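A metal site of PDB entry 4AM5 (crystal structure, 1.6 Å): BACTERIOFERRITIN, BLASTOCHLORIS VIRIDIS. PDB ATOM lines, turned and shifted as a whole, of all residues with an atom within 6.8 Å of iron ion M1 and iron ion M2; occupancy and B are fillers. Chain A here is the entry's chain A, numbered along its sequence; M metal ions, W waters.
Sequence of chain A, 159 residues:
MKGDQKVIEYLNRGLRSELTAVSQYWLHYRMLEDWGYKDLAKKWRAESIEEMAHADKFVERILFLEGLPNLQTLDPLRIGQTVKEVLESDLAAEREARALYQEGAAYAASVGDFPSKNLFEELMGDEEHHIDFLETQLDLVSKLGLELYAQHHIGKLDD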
ATOM      1  N   SER A  17      26.519 -23.854  13.610  1.00  0.00           N
ATOM      2  CA  SER A  17      26.557 -22.410  13.827  1.00  0.00           C
ATOM      3  C   SER A  17      25.384 -21.682  13.162  1.00  0.00           C
ATOM      4  O   SER A  17      24.750 -20.829  13.815  1.00  0.00           O
ATOM      5  CB  SER A  17      27.893 -21.915  13.304  1.00  0.00           C
ATOM      6  OG  SER A  17      28.010 -20.570  13.793  1.00  0.00           O
ATOM      7  N   GLU A  18      25.126 -22.037  11.893  1.00  0.00           N
ATOM      8  CA  GLU A  18      24.030 -21.357  11.214  1.00  0.00           C
ATOM      9  C   GLU A  18      22.661 -21.720  11.758  1.00  0.00           C
ATOM     10  O   GLU A  18      21.805 -20.866  11.843  1.00  0.00           O
ATOM     11  CB  GLU A  18      24.053 -21.701   9.724  1.00  0.00           C
ATOM     12  CG  GLU A  18      25.256 -21.149   8.993  1.00  0.00           C
ATOM     13  CD  GLU A  18      25.289 -19.634   8.920  1.00  0.00           C
ATOM     14  OE1 GLU A  18      24.253 -19.001   9.040  1.00  0.00           O
ATOM     15  OE2 GLU A  18      26.347 -19.066   8.628  1.00  0.00           O
ATOM     16  N   ALA A  21      22.253 -19.489  14.578  1.00  0.00           N
ATOM     17  CA  ALA A  21      21.942 -18.111  14.181  1.00  0.00           C
ATOM     18  C   ALA A  21      20.527 -17.978  13.693  1.00  0.00           C
ATOM     19  O   ALA A  21      19.876 -16.962  13.948  1.00  0.00           O
ATOM     20  CB  ALA A  21      22.893 -17.677  13.067  1.00  0.00           C
ATOM     21  N   TYR A  25      18.366 -15.368  15.783  1.00  0.00           N
ATOM     22  CA  TYR A  25      17.725 -14.208  15.123  1.00  0.00           C
ATOM     23  C   TYR A  25      16.212 -14.341  15.056  1.00  0.00           C
ATOM     24  O   TYR A  25      15.522 -13.287  15.172  1.00  0.00           O
ATOM     25  CB  TYR A  25      18.296 -14.045  13.678  1.00  0.00           C
ATOM     26  CG  TYR A  25      19.618 -13.320  13.569  1.00  0.00           C
ATOM     27  CD1 TYR A  25      19.738 -12.000  14.031  1.00  0.00           C
ATOM     28  CD2 TYR A  25      20.706 -13.941  12.947  1.00  0.00           C
ATOM     29  CE1 TYR A  25      20.948 -11.316  13.895  1.00  0.00           C
ATOM     30  CE2 TYR A  25      21.950 -13.276  12.838  1.00  0.00           C
ATOM     31  CZ  TYR A  25      22.061 -11.990  13.290  1.00  0.00           C
ATOM     32  OH  TYR A  25      23.255 -11.306  13.061  1.00  0.00           O
ATOM     33  N   GLU A  47      17.476 -10.973   8.645  1.00  0.00           N
ATOM     34  CA  GLU A  47      18.798 -11.582   8.932  1.00  0.00           C
ATOM     35  C   GLU A  47      18.653 -13.074   9.201  1.00  0.00           C
ATOM     36  O   GLU A  47      19.489 -13.865   8.756  1.00  0.00           O
ATOM     37  CB  GLU A  47      19.488 -10.931  10.145  1.00  0.00           C
ATOM     38  CG  GLU A  47      19.745  -9.465   9.876  1.00  0.00           C
ATOM     39  CD  GLU A  47      20.922  -9.236   8.900  1.00  0.00           C
ATOM     40  OE1 GLU A  47      21.187 -10.032   7.936  1.00  0.00           O
ATOM     41  OE2 GLU A  47      21.659  -8.205   9.243  1.00  0.00           O
ATOM     42  N   GLU A  50      18.478 -14.770   5.931  1.00  0.00           N
ATOM     43  CA  GLU A  50      19.848 -14.851   5.297  1.00  0.00           C
ATOM     44  C   GLU A  50      20.578 -16.068   5.941  1.00  0.00           C
ATOM     45  O   GLU A  50      21.302 -16.790   5.211  1.00  0.00           O
ATOM     46  CB  GLU A  50      20.685 -13.580   5.575  1.00  0.00           C
ATOM     47  CG  GLU A  50      20.124 -12.409   4.819  1.00  0.00           C
ATOM     48  CD  GLU A  50      21.019 -11.178   4.868  1.00  0.00           C
ATOM     49  OE1 GLU A  50      22.287 -11.310   5.037  1.00  0.00           O
ATOM     50  OE2 GLU A  50      20.430 -10.103   4.529  1.00  0.00           O
ATOM     51  N   GLU A  51      20.447 -16.289   7.268  1.00  0.00           N
ATOM     52  CA  GLU A  51      21.240 -17.406   7.864  1.00  0.00           C
ATOM     53  C   GLU A  51      20.599 -18.730   7.400  1.00  0.00           C
ATOM     54  O   GLU A  51      21.291 -19.754   7.329  1.00  0.00           O
ATOM     55  CB  GLU A  51      21.217 -17.333   9.414  1.00  0.00           C
ATOM     56  CG  GLU A  51      21.746 -16.012  10.005  1.00  0.00           C
ATOM     57  CD  GLU A  51      23.078 -15.560   9.648  1.00  0.00           C
ATOM     58  OE1 GLU A  51      23.645 -15.985   8.687  1.00  0.00           O
ATOM     59  OE2 GLU A  51      23.582 -14.769  10.442  1.00  0.00           O
ATOM     60  N   MET A  52      19.282 -18.775   7.121  1.00  0.00           N
ATOM     61  CA  MET A  52      18.638 -20.000   6.632  1.00  0.00           C
ATOM     62  C   MET A  52      19.336 -20.363   5.282  1.00  0.00           C
ATOM     63  O   MET A  52      19.575 -21.585   5.029  1.00  0.00           O
ATOM     64  CB  MET A  52      17.125 -19.795   6.421  1.00  0.00           C
ATOM     65  CG  MET A  52      16.395 -19.640   7.805  1.00  0.00           C
ATOM     66  SD  MET A  52      14.662 -19.232   7.443  1.00  0.00           S
ATOM     67  CE  MET A  52      14.260 -18.369   8.995  1.00  0.00           C
ATOM     68  N   HIS A  54      22.369 -19.695   4.369  1.00  0.00           N
ATOM     69  CA  HIS A  54      23.718 -20.204   4.707  1.00  0.00           C
ATOM     70  C   HIS A  54      23.626 -21.641   5.217  1.00  0.00           C
ATOM     71  O   HIS A  54      24.441 -22.492   4.806  1.00  0.00           O
ATOM     72  CB  HIS A  54      24.299 -19.423   5.859  1.00  0.00           C
ATOM     73  CG  HIS A  54      24.744 -18.022   5.519  1.00  0.00           C
ATOM     74  ND1 HIS A  54      25.230 -17.066   6.494  1.00  0.00           N
ATOM     75  CD2 HIS A  54      24.931 -17.471   4.270  1.00  0.00           C
ATOM     76  CE1 HIS A  54      25.653 -15.961   5.759  1.00  0.00           C
ATOM     77  NE2 HIS A  54      25.426 -16.169   4.463  1.00  0.00           N
ATOM     78  N   ALA A  55      22.662 -21.955   6.096  1.00  0.00           N
ATOM     79  CA  ALA A  55      22.514 -23.344   6.591  1.00  0.00           C
ATOM     80  C   ALA A  55      22.298 -24.280   5.396  1.00  0.00           C
ATOM     81  O   ALA A  55      22.911 -25.370   5.348  1.00  0.00           O
ATOM     82  CB  ALA A  55      21.342 -23.385   7.570  1.00  0.00           C
ATOM     83  N   PHE A  58      25.403 -25.133   3.548  1.00  0.00           N
ATOM     84  CA  PHE A  58      26.232 -26.196   4.171  1.00  0.00           C
ATOM     85  C   PHE A  58      25.648 -27.572   3.975  1.00  0.00           C
ATOM     86  O   PHE A  58      26.405 -28.523   3.709  1.00  0.00           O
ATOM     87  CB  PHE A  58      26.410 -25.908   5.682  1.00  0.00           C
ATOM     88  CG  PHE A  58      27.428 -24.842   5.983  1.00  0.00           C
ATOM     89  CD1 PHE A  58      28.718 -24.928   5.476  1.00  0.00           C
ATOM     90  CD2 PHE A  58      27.112 -23.782   6.863  1.00  0.00           C
ATOM     91  CE1 PHE A  58      29.697 -23.987   5.824  1.00  0.00           C
ATOM     92  CE2 PHE A  58      28.103 -22.844   7.239  1.00  0.00           C
ATOM     93  CZ  PHE A  58      29.414 -22.936   6.673  1.00  0.00           C
ATOM     94  N   GLU A  94      27.834 -13.958  16.249  1.00  0.00           N
ATOM     95  CA  GLU A  94      28.358 -13.769  14.891  1.00  0.00           C
ATOM     96  C   GLU A  94      29.907 -13.687  14.861  1.00  0.00           C
ATOM     97  O   GLU A  94      30.491 -14.161  13.896  1.00  0.00           O
ATOM     98  CB  GLU A  94      27.695 -12.513  14.322  1.00  0.00           C
ATOM     99  CG  GLU A  94      26.166 -12.686  14.227  1.00  0.00           C
ATOM    100  CD  GLU A  94      25.727 -13.443  12.976  1.00  0.00           C
ATOM    101  OE1 GLU A  94      25.855 -14.711  12.949  1.00  0.00           O
ATOM    102  OE2 GLU A  94      25.273 -12.713  12.015  1.00  0.00           O
ATOM    103  N   ALA A  97      30.906 -17.247  14.728  1.00  0.00           N
ATOM    104  CA  ALA A  97      30.764 -17.800  13.373  1.00  0.00           C
ATOM    105  C   ALA A  97      31.874 -17.386  12.405  1.00  0.00           C
ATOM    106  O   ALA A  97      32.389 -18.211  11.656  1.00  0.00           O
ATOM    107  CB  ALA A  97      29.370 -17.403  12.819  1.00  0.00           C
ATOM    108  N   TYR A 101      34.499 -19.772  10.398  1.00  0.00           N
ATOM    109  CA  TYR A 101      34.690 -19.830   8.949  1.00  0.00           C
ATOM    110  C   TYR A 101      36.083 -19.472   8.464  1.00  0.00           C
ATOM    111  O   TYR A 101      36.540 -20.020   7.422  1.00  0.00           O
ATOM    112  CB  TYR A 101      33.601 -18.903   8.246  1.00  0.00           C
ATOM    113  CG  TYR A 101      32.184 -19.330   8.615  1.00  0.00           C
ATOM    114  CD1 TYR A 101      31.905 -20.555   9.145  1.00  0.00           C
ATOM    115  CD2 TYR A 101      31.129 -18.407   8.469  1.00  0.00           C
ATOM    116  CE1 TYR A 101      30.632 -20.895   9.584  1.00  0.00           C
ATOM    117  CE2 TYR A 101      29.812 -18.729   8.830  1.00  0.00           C
ATOM    118  CZ  TYR A 101      29.566 -19.969   9.408  1.00  0.00           C
ATOM    119  OH  TYR A 101      28.273 -20.256   9.762  1.00  0.00           O
ATOM    120  N   LEU A 123      30.903 -17.024   3.214  1.00  0.00           N
ATOM    121  CA  LEU A 123      30.122 -16.834   4.454  1.00  0.00           C
ATOM    122  C   LEU A 123      30.915 -15.965   5.432  1.00  0.00           C
ATOM    123  O   LEU A 123      30.271 -15.187   6.195  1.00  0.00           O
ATOM    124  CB  LEU A 123      29.754 -18.212   5.056  1.00  0.00           C
ATOM    125  CG  LEU A 123      28.359 -18.670   4.498  1.00  0.00           C
ATOM    126  CD1 LEU A 123      28.171 -18.622   3.011  1.00  0.00           C
ATOM    127  CD2 LEU A 123      28.123 -20.126   4.964  1.00  0.00           C
ATOM    128  N   ASP A 126      30.054 -12.577   4.578  1.00  0.00           N
ATOM    129  CA  ASP A 126      28.709 -12.180   4.924  1.00  0.00           C
ATOM    130  C   ASP A 126      28.564 -11.974   6.438  1.00  0.00           C
ATOM    131  O   ASP A 126      27.863 -11.070   6.828  1.00  0.00           O
ATOM    132  CB  ASP A 126      27.788 -13.340   4.559  1.00  0.00           C
ATOM    133  CG  ASP A 126      27.609 -13.539   3.080  1.00  0.00           C
ATOM    134  OD1 ASP A 126      27.879 -12.590   2.254  1.00  0.00           O
ATOM    135  OD2 ASP A 126      27.040 -14.628   2.671  1.00  0.00           O
ATOM    136  N   GLU A 127      29.264 -12.816   7.234  1.00  0.00           N
ATOM    137  CA  GLU A 127      29.152 -12.596   8.668  1.00  0.00           C
ATOM    138  C   GLU A 127      29.881 -11.307   9.066  1.00  0.00           C
ATOM    139  O   GLU A 127      29.416 -10.653  10.072  1.00  0.00           O
ATOM    140  CB  GLU A 127      29.726 -13.746   9.523  1.00  0.00           C
ATOM    141  CG  GLU A 127      29.097 -15.094   9.193  1.00  0.00           C
ATOM    142  CD  GLU A 127      27.581 -15.028   9.140  1.00  0.00           C
ATOM    143  OE1 GLU A 127      26.981 -14.256   9.932  1.00  0.00           O
ATOM    144  OE2 GLU A 127      27.156 -16.001   8.508  1.00  0.00           O
ATOM    145  N   GLU A 128      30.952 -10.873   8.368  1.00  0.00           N
ATOM    146  CA  GLU A 128      31.500  -9.575   8.750  1.00  0.00           C
ATOM    147  C   GLU A 128      30.524  -8.429   8.419  1.00  0.00           C
ATOM    148  O   GLU A 128      30.493  -7.466   9.159  1.00  0.00           O
ATOM    149  CB  GLU A 128      32.826  -9.374   8.003  1.00  0.00           C
ATOM    150  CG  GLU A 128      33.949 -10.185   8.729  1.00  0.00           C
ATOM    151  CD  GLU A 128      35.320  -9.973   8.214  1.00  0.00           C
ATOM    152  OE1 GLU A 128      35.525  -9.079   7.393  1.00  0.00           O
ATOM    153  OE2 GLU A 128      36.263 -10.645   8.726  1.00  0.00           O
ATOM    154  N   HIS A 130      27.227  -8.784   8.753  1.00  0.00           N
ATOM    155  CA  HIS A 130      26.325  -8.811   9.928  1.00  0.00           C
ATOM    156  C   HIS A 130      26.943  -8.216  11.159  1.00  0.00           C
ATOM    157  O   HIS A 130      26.268  -7.518  11.922  1.00  0.00           O
ATOM    158  CB  HIS A 130      25.919 -10.272  10.237  1.00  0.00           C
ATOM    159  CG  HIS A 130      25.098 -10.899   9.140  1.00  0.00           C
ATOM    160  ND1 HIS A 130      24.847 -12.275   9.045  1.00  0.00           N
ATOM    161  CD2 HIS A 130      24.546 -10.309   7.988  1.00  0.00           C
ATOM    162  CE1 HIS A 130      24.124 -12.512   7.909  1.00  0.00           C
ATOM    163  NE2 HIS A 130      23.938 -11.342   7.250  1.00  0.00           N
ATOM    164  N   ILE A 131      28.234  -8.493  11.413  1.00  0.00           N
ATOM    165  CA  ILE A 131      28.984  -7.893  12.510  1.00  0.00           C
ATOM    166  C   ILE A 131      28.976  -6.337  12.375  1.00  0.00           C
ATOM    167  O   ILE A 131      28.765  -5.646  13.381  1.00  0.00           O
ATOM    168  CB  ILE A 131      30.442  -8.475  12.545  1.00  0.00           C
ATOM    169  CG1 ILE A 131      30.316  -9.888  13.115  1.00  0.00           C
ATOM    170  CG2 ILE A 131      31.377  -7.632  13.436  1.00  0.00           C
ATOM    171  CD1 ILE A 131      31.595 -10.690  12.801  1.00  0.00           C
ATOM    172  N   LEU A 134      25.606  -4.986  13.463  1.00  0.00           N
ATOM    173  CA  LEU A 134      25.401  -5.062  14.877  1.00  0.00           C
ATOM    174  C   LEU A 134      26.308  -4.106  15.682  1.00  0.00           C
ATOM    175  O   LEU A 134      25.807  -3.416  16.583  1.00  0.00           O
ATOM    176  CB  LEU A 134      25.675  -6.474  15.415  1.00  0.00           C
ATOM    177  CG  LEU A 134      24.639  -7.467  14.850  1.00  0.00           C
ATOM    178  CD1 LEU A 134      25.120  -8.984  15.016  1.00  0.00           C
ATOM    179  CD2 LEU A 134      23.190  -7.307  15.448  1.00  0.00           C
HETATM  180 FE    FE M   1      25.279 -13.754  10.321  1.00  0.00          FE
HETATM  181 FE    FE M   2      25.371 -17.133   8.548  1.00  0.00          FE
HETATM  182  O   HOH W   1      25.557 -17.027  10.923  1.00  0.00           O
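NE2 of His 130 lies within hydrogen-bond range of OE1 of Glu 50.
The side-chain hydroxyl (OH) of Tyr 25 sits close to the side-chain carboxylate (OE2) of Glu 94 (2.7 Å).
The side-chain carboxylate of Asp 126 is in hydrogen-bond range of a ring nitrogen (NE2) of His 54 (2.9 Å).
NE2 of His 130 lies within hydrogen-bond range of OE1 of Glu 47, at 3.1 Å.
OE2 of Glu 18 sits close to OH of Tyr 101 (2.5 Å).
Within 4 Å of iron ion M2: Glu 18, Glu 51, His 54 and Glu 127.
Iron ion M1 is bound by OE1 of Glu 127 (1.8 Å), OE2 of Glu 51 (2.0 Å), OE2 of Glu 94 (2.0 Å) and ND1 of His 130 (2.0 Å).
Iron ion M2 is bound by ND1 of His 54, OE1 of Glu 51, OE2 of Glu 127, OE2 of Glu 18, OE1 of Glu 18 and water W1.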
